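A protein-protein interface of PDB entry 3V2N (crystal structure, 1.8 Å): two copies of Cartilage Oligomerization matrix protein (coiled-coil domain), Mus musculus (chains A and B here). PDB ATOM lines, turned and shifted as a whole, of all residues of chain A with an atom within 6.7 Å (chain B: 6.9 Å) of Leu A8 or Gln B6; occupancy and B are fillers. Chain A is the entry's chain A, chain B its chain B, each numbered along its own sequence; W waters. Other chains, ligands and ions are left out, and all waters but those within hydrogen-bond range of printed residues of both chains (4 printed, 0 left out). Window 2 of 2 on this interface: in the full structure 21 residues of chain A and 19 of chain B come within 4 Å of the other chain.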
ATOM      1  N   LEU A   3      15.634  19.922  -5.850  1.00  0.00           N
ATOM      2  CA  LEU A   3      15.769  19.877  -4.397  1.00  0.00           C
ATOM      3  C   LEU A   3      14.620  20.529  -3.627  1.00  0.00           C
ATOM      4  O   LEU A   3      14.604  20.490  -2.394  1.00  0.00           O
ATOM      5  CB  LEU A   3      17.088  20.539  -3.975  1.00  0.00           C
ATOM      6  CG  LEU A   3      18.429  19.890  -4.329  1.00  0.00           C
ATOM      7  CD1 LEU A   3      18.514  19.586  -5.811  1.00  0.00           C
ATOM      8  CD2 LEU A   3      19.551  20.832  -3.924  1.00  0.00           C
ATOM      9  N   ALA A   4      13.665  21.127  -4.339  1.00  0.00           N
ATOM     10  CA  ALA A   4      12.524  21.773  -3.686  1.00  0.00           C
ATOM     11  C   ALA A   4      11.756  20.811  -2.781  1.00  0.00           C
ATOM     12  O   ALA A   4      11.432  21.148  -1.646  1.00  0.00           O
ATOM     13  CB  ALA A   4      11.573  22.369  -4.730  1.00  0.00           C
ATOM     14  N   PRO A   5      11.447  19.601  -3.273  1.00  0.00           N
ATOM     15  CA  PRO A   5      10.709  18.671  -2.411  1.00  0.00           C
ATOM     16  C   PRO A   5      11.476  18.372  -1.132  1.00  0.00           C
ATOM     17  O   PRO A   5      10.895  18.291  -0.054  1.00  0.00           O
ATOM     18  CB  PRO A   5      10.534  17.443  -3.300  1.00  0.00           C
ATOM     19  CG  PRO A   5      10.455  18.056  -4.679  1.00  0.00           C
ATOM     20  CD  PRO A   5      11.597  19.044  -4.627  1.00  0.00           C
ATOM     21  N   GLN A   6      12.787  18.215  -1.259  1.00  0.00           N
ATOM     22  CA  GLN A   6      13.616  17.934  -0.096  1.00  0.00           C
ATOM     23  C   GLN A   6      13.639  19.129   0.865  1.00  0.00           C
ATOM     24  O   GLN A   6      13.607  18.960   2.087  1.00  0.00           O
ATOM     25  CB  GLN A   6      15.030  17.570  -0.537  1.00  0.00           C
ATOM     26  CG  GLN A   6      15.909  17.117   0.607  1.00  0.00           C
ATOM     27  CD  GLN A   6      17.044  16.227   0.154  1.00  0.00           C
ATOM     28  OE1 GLN A   6      17.905  15.858   0.947  1.00  0.00           O
ATOM     29  NE2 GLN A   6      17.048  15.869  -1.125  1.00  0.00           N
ATOM     30  N   MET A   7      13.681  20.339   0.317  1.00  0.00           N
ATOM     31  CA  MET A   7      13.679  21.528   1.160  1.00  0.00           C
ATOM     32  C   MET A   7      12.372  21.603   1.945  1.00  0.00           C
ATOM     33  O   MET A   7      12.366  21.940   3.129  1.00  0.00           O
ATOM     34  CB  MET A   7      13.856  22.795   0.308  1.00  0.00           C
ATOM     35  CG  MET A   7      15.224  22.891  -0.362  1.00  0.00           C
ATOM     36  SD  MET A   7      15.482  24.418  -1.302  1.00  0.00           S
ATOM     37  CE  MET A   7      15.254  25.632  -0.006  1.00  0.00           C
ATOM     38  N   LEU A   8      11.263  21.276   1.283  1.00  0.00           N
ATOM     39  CA  LEU A   8       9.959  21.321   1.928  1.00  0.00           C
ATOM     40  C   LEU A   8       9.933  20.328   3.088  1.00  0.00           C
ATOM     41  O   LEU A   8       9.450  20.644   4.173  1.00  0.00           O
ATOM     42  CB  LEU A   8       8.853  21.001   0.916  1.00  0.00           C
ATOM     43  CG  LEU A   8       7.418  21.019   1.439  1.00  0.00           C
ATOM     44  CD1 LEU A   8       7.077  22.384   2.028  1.00  0.00           C
ATOM     45  CD2 LEU A   8       6.467  20.681   0.307  1.00  0.00           C
ATOM     46  N   ARG A   9      10.481  19.140   2.861  1.00  0.00           N
ATOM     47  CA  ARG A   9      10.534  18.118   3.902  1.00  0.00           C
ATOM     48  C   ARG A   9      11.341  18.598   5.109  1.00  0.00           C
ATOM     49  O   ARG A   9      10.947  18.368   6.255  1.00  0.00           O
ATOM     50  CB  ARG A   9      11.119  16.816   3.342  1.00  0.00           C
ATOM     51  CG  ARG A   9      10.078  15.941   2.639  1.00  0.00           C
ATOM     52  CD  ARG A   9       9.009  15.483   3.633  1.00  0.00           C
ATOM     53  NE  ARG A   9       9.538  14.505   4.578  1.00  0.00           N
ATOM     54  CZ  ARG A   9       9.306  14.513   5.887  1.00  0.00           C
ATOM     55  NH1 ARG A   9       8.546  15.454   6.431  1.00  0.00           N
ATOM     56  NH2 ARG A   9       9.839  13.578   6.654  1.00  0.00           N
ATOM     57  N   GLU A  10      12.456  19.278   4.856  1.00  0.00           N
ATOM     58  CA  GLU A  10      13.274  19.786   5.954  1.00  0.00           C
ATOM     59  C   GLU A  10      12.450  20.780   6.783  1.00  0.00           C
ATOM     60  O   GLU A  10      12.435  20.714   8.011  1.00  0.00           O
ATOM     61  CB  GLU A  10      14.537  20.480   5.424  1.00  0.00           C
ATOM     62  CG  GLU A  10      15.584  19.565   4.791  1.00  0.00           C
ATOM     63  CD  GLU A  10      16.150  18.538   5.767  1.00  0.00           C
ATOM     64  OE1 GLU A  10      16.204  18.829   6.982  1.00  0.00           O
ATOM     65  OE2 GLU A  10      16.555  17.447   5.317  1.00  0.00           O
ATOM     66  N   LEU A  11      11.757  21.692   6.103  1.00  0.00           N
ATOM     67  CA  LEU A  11      10.918  22.685   6.779  1.00  0.00           C
ATOM     68  C   LEU A  11       9.839  21.986   7.609  1.00  0.00           C
ATOM     69  O   LEU A  11       9.526  22.409   8.726  1.00  0.00           O
ATOM     70  CB  LEU A  11      10.254  23.612   5.754  1.00  0.00           C
ATOM     71  CG  LEU A  11      11.160  24.447   4.841  1.00  0.00           C
ATOM     72  CD1 LEU A  11      10.303  25.372   3.990  1.00  0.00           C
ATOM     73  CD2 LEU A  11      12.133  25.260   5.679  1.00  0.00           C
ATOM     74  N   GLN A  12       9.262  20.918   7.059  1.00  0.00           N
ATOM     75  CA  GLN A  12       8.235  20.171   7.774  1.00  0.00           C
ATOM     76  C   GLN A  12       8.811  19.494   9.012  1.00  0.00           C
ATOM     77  O   GLN A  12       8.140  19.399  10.045  1.00  0.00           O
ATOM     78  CB  GLN A  12       7.597  19.119   6.864  1.00  0.00           C
ATOM     79  CG  GLN A  12       6.745  19.696   5.750  1.00  0.00           C
ATOM     80  CD  GLN A  12       6.138  18.611   4.885  1.00  0.00           C
ATOM     81  OE1 GLN A  12       6.843  17.717   4.415  1.00  0.00           O
ATOM     82  NE2 GLN A  12       4.830  18.684   4.666  1.00  0.00           N
ATOM     83  N   GLU A  13      10.045  19.010   8.904  1.00  0.00           N
ATOM     84  CA  GLU A  13      10.702  18.362  10.031  1.00  0.00           C
ATOM     85  C   GLU A  13      11.036  19.403  11.094  1.00  0.00           C
ATOM     86  O   GLU A  13      10.984  19.122  12.288  1.00  0.00           O
ATOM     87  CB  GLU A  13      11.972  17.640   9.572  1.00  0.00           C
ATOM     88  CG  GLU A  13      11.707  16.283   8.947  1.00  0.00           C
ATOM     89  CD  GLU A  13      10.986  15.352   9.906  1.00  0.00           C
ATOM     90  OE1 GLU A  13      11.471  15.190  11.043  1.00  0.00           O
ATOM     91  OE2 GLU A  13       9.936  14.792   9.528  1.00  0.00           O
ATOM     92  N   MET B   1       5.872  20.846 -10.146  1.00  0.00           N
ATOM     93  CA  MET B   1       4.813  21.483  -9.314  1.00  0.00           C
ATOM     94  C   MET B   1       5.390  22.503  -8.344  1.00  0.00           C
ATOM     95  O   MET B   1       6.276  22.190  -7.546  1.00  0.00           O
ATOM     96  CB  MET B   1       4.038  20.412  -8.544  1.00  0.00           C
ATOM     97  CG  MET B   1       2.634  20.183  -9.074  1.00  0.00           C
ATOM     98  SD  MET B   1       2.588  20.100 -10.878  1.00  0.00           S
ATOM     99  CE  MET B   1       1.949  21.741 -11.279  1.00  0.00           C
ATOM    100  N   ASP B   2       4.874  23.724  -8.418  1.00  0.00           N
ATOM    101  CA  ASP B   2       5.331  24.812  -7.562  1.00  0.00           C
ATOM    102  C   ASP B   2       5.068  24.537  -6.079  1.00  0.00           C
ATOM    103  O   ASP B   2       3.916  24.469  -5.636  1.00  0.00           O
ATOM    104  CB  ASP B   2       4.657  26.114  -8.002  1.00  0.00           C
ATOM    105  CG  ASP B   2       4.967  27.272  -7.088  1.00  0.00           C
ATOM    106  OD1 ASP B   2       6.148  27.449  -6.719  1.00  0.00           O
ATOM    107  OD2 ASP B   2       4.025  28.014  -6.745  1.00  0.00           O
ATOM    108  N   LEU B   3       6.148  24.374  -5.317  1.00  0.00           N
ATOM    109  CA  LEU B   3       6.044  24.097  -3.890  1.00  0.00           C
ATOM    110  C   LEU B   3       6.156  25.350  -3.029  1.00  0.00           C
ATOM    111  O   LEU B   3       6.126  25.267  -1.805  1.00  0.00           O
ATOM    112  CB  LEU B   3       7.121  23.093  -3.470  1.00  0.00           C
ATOM    113  CG  LEU B   3       7.066  21.743  -4.189  1.00  0.00           C
ATOM    114  CD1 LEU B   3       8.149  20.819  -3.632  1.00  0.00           C
ATOM    115  CD2 LEU B   3       5.682  21.125  -4.006  1.00  0.00           C
ATOM    116  N   ALA B   4       6.290  26.503  -3.677  1.00  0.00           N
ATOM    117  CA  ALA B   4       6.399  27.777  -2.975  1.00  0.00           C
ATOM    118  C   ALA B   4       5.233  28.011  -2.016  1.00  0.00           C
ATOM    119  O   ALA B   4       5.435  28.428  -0.880  1.00  0.00           O
ATOM    120  CB  ALA B   4       6.486  28.925  -3.979  1.00  0.00           C
ATOM    121  N   PRO B   5       3.992  27.759  -2.464  1.00  0.00           N
ATOM    122  CA  PRO B   5       2.840  27.969  -1.582  1.00  0.00           C
ATOM    123  C   PRO B   5       2.921  27.140  -0.304  1.00  0.00           C
ATOM    124  O   PRO B   5       2.634  27.637   0.788  1.00  0.00           O
ATOM    125  CB  PRO B   5       1.659  27.564  -2.462  1.00  0.00           C
ATOM    126  CG  PRO B   5       2.132  27.918  -3.836  1.00  0.00           C
ATOM    127  CD  PRO B   5       3.553  27.414  -3.827  1.00  0.00           C
ATOM    128  N   GLN B   6       3.314  25.878  -0.440  1.00  0.00           N
ATOM    129  CA  GLN B   6       3.434  24.999   0.717  1.00  0.00           C
ATOM    130  C   GLN B   6       4.603  25.429   1.606  1.00  0.00           C
ATOM    131  O   GLN B   6       4.498  25.395   2.828  1.00  0.00           O
ATOM    132  CB  GLN B   6       3.616  23.546   0.274  1.00  0.00           C
ATOM    133  CG  GLN B   6       2.379  22.951  -0.401  1.00  0.00           C
ATOM    134  CD  GLN B   6       2.564  21.496  -0.793  1.00  0.00           C
ATOM    135  OE1 GLN B   6       2.655  20.614   0.065  1.00  0.00           O
ATOM    136  NE2 GLN B   6       2.626  21.238  -2.093  1.00  0.00           N
ATOM    137  N   MET B   7       5.712  25.836   0.993  1.00  0.00           N
ATOM    138  CA  MET B   7       6.870  26.274   1.774  1.00  0.00           C
ATOM    139  C   MET B   7       6.514  27.496   2.613  1.00  0.00           C
ATOM    140  O   MET B   7       6.875  27.569   3.789  1.00  0.00           O
ATOM    141  CB  MET B   7       8.046  26.606   0.861  1.00  0.00           C
ATOM    142  CG  MET B   7       8.764  25.391   0.313  1.00  0.00           C
ATOM    143  SD  MET B   7      10.063  25.854  -0.827  1.00  0.00           S
ATOM    144  CE  MET B   7      11.434  26.097   0.289  1.00  0.00           C
ATOM    145  N   LEU B   8       5.802  28.445   2.004  1.00  0.00           N
ATOM    146  CA  LEU B   8       5.390  29.660   2.698  1.00  0.00           C
ATOM    147  C   LEU B   8       4.572  29.290   3.933  1.00  0.00           C
ATOM    148  O   LEU B   8       4.808  29.825   5.013  1.00  0.00           O
ATOM    149  CB  LEU B   8       4.566  30.566   1.769  1.00  0.00           C
ATOM    150  CG  LEU B   8       3.946  31.808   2.421  1.00  0.00           C
ATOM    151  CD1 LEU B   8       5.027  32.643   3.071  1.00  0.00           C
ATOM    152  CD2 LEU B   8       3.200  32.628   1.383  1.00  0.00           C
ATOM    153  N   ARG B   9       3.622  28.370   3.777  1.00  0.00           N
ATOM    154  CA  ARG B   9       2.803  27.950   4.911  1.00  0.00           C
ATOM    155  C   ARG B   9       3.658  27.380   6.051  1.00  0.00           C
ATOM    156  O   ARG B   9       3.370  27.609   7.225  1.00  0.00           O
ATOM    157  CB  ARG B   9       1.746  26.925   4.471  1.00  0.00           C
ATOM    158  CG  ARG B   9       0.485  27.571   3.889  1.00  0.00           C
ATOM    159  CD  ARG B   9      -0.701  26.604   3.850  1.00  0.00           C
ATOM    160  NE  ARG B   9      -0.583  25.583   2.811  1.00  0.00           N
ATOM    161  CZ  ARG B   9      -0.734  25.812   1.509  1.00  0.00           C
ATOM    162  NH1 ARG B   9      -0.605  24.816   0.643  1.00  0.00           N
ATOM    163  NH2 ARG B   9      -1.022  27.032   1.071  1.00  0.00           N
ATOM    164  N   GLU B  10       4.707  26.642   5.706  1.00  0.00           N
ATOM    165  CA  GLU B  10       5.597  26.070   6.717  1.00  0.00           C
ATOM    166  C   GLU B  10       6.344  27.194   7.443  1.00  0.00           C
ATOM    167  O   GLU B  10       6.487  27.158   8.660  1.00  0.00           O
ATOM    168  CB  GLU B  10       6.603  25.111   6.070  1.00  0.00           C
ATOM    169  CG  GLU B  10       5.982  23.843   5.503  1.00  0.00           C
ATOM    170  CD  GLU B  10       5.248  23.027   6.559  1.00  0.00           C
ATOM    171  OE1 GLU B  10       5.849  22.730   7.609  1.00  0.00           O
ATOM    172  OE2 GLU B  10       4.073  22.675   6.338  1.00  0.00           O
ATOM    173  N   LEU B  11       6.814  28.188   6.696  1.00  0.00           N
ATOM    174  CA  LEU B  11       7.531  29.311   7.299  1.00  0.00           C
ATOM    175  C   LEU B  11       6.595  30.104   8.213  1.00  0.00           C
ATOM    176  O   LEU B  11       7.012  30.637   9.239  1.00  0.00           O
ATOM    177  CB  LEU B  11       8.082  30.238   6.217  1.00  0.00           C
ATOM    178  CG  LEU B  11       9.107  29.649   5.243  1.00  0.00           C
ATOM    179  CD1 LEU B  11       9.520  30.731   4.252  1.00  0.00           C
ATOM    180  CD2 LEU B  11      10.323  29.123   6.005  1.00  0.00           C
HETATM  181  O   HOH W   1       2.700  20.678   2.969  1.00  0.00           O
HETATM  182  O   HOH W   2      10.860  23.203  -0.500  1.00  0.00           O
HETATM  183  O   HOH W   3       9.507  25.485   8.405  1.00  0.00           O
HETATM  184  O   HOH W   4       2.426  20.570   6.352  1.00  0.00           O
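OE1 of Gln A12 sits close to NH1 of Arg A9.
Among the printed residues, pairs that only touch across the chains: Ala A4 with Leu B3 (3.7 Å), Pro A5 with Leu B3 (3.5 Å), Met A7 with Met B7 (3.9 Å), Leu A8 with Gln B6 (3.8 Å), Leu A8 with Met B7 (3.9 Å), Leu A8 with Glu B10 (3.9 Å), Leu A11 with Met B7 (3.9 Å), Leu A11 with Glu B10 (3.9 Å) and Gln A12 with Glu B10 (3.5 Å).
Of the printed residues of chain B, Met A7 touches Met B7 (3.9 Å). Of chain B, only Gln B6 (3.8 Å), Met B7 (3.9 Å) and Glu B10 (3.9 Å) come within 4 Å of Leu A8. Of the printed residues of chain B, Gln A12 touches Glu B10 (3.5 Å). Leu B8 touches none of the printed residues of chain A. The nearest residue of chain B that does not touch Leu A8 is Leu B3 (4.3 Å). The nearest residue of chain A that does not touch Gln B6 is Gln A12 (5.4 Å).
Hydrophobic or aromatic side chains of chain A within 4 Å of the printed part of chain B: Ala A4, Pro A5, Met A7, Leu A8 and Leu A11. Of the 11 printed residues of chain B, 4 touch a printed residue of chain A. Along chain B the printed residues that touch a printed residue of chain A span positions 3 to 10. Among the printed residues, 9 pairs touch across the chains. Among the printed residues, no Asp or Glu carboxylate lies within 4 Å of a Lys or Arg side-chain nitrogen of the other chain.
Met A7 touches its own counterpart, Met B7. Leu A8 touches Gln B6, but with the chains exchanged Gln A6 does not touch Leu B8 (12.2 Å). Leu A8 touches Met B7, but with the chains exchanged Met A7 does not touch Leu B8 (9.3 Å). Leu A8 touches Glu B10, but with the chains exchanged Glu A10 does not touch Leu B8 (11.2 Å). Of the 9 pairs that touch across the chains among the printed residues, 1 has its exchanged pair printed and touching as well.
Water W2 lies within hydrogen-bond range of O of Ala A4, N of Leu A8 and SD of Met B7. Water W4 lies within hydrogen-bond range of OE2 of Glu B10 (2.7 Å) and NE2 of Gln A12 (3.5 Å). Water W1 lies within hydrogen-bond range of OE1 of Gln B6 and NE2 of Gln A12. Water W3 lies within hydrogen-bond range of the backbone carbonyl oxygen of Leu A11 (3.1 Å) and the backbone carbonyl oxygen of Glu B10 (3.5 Å).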
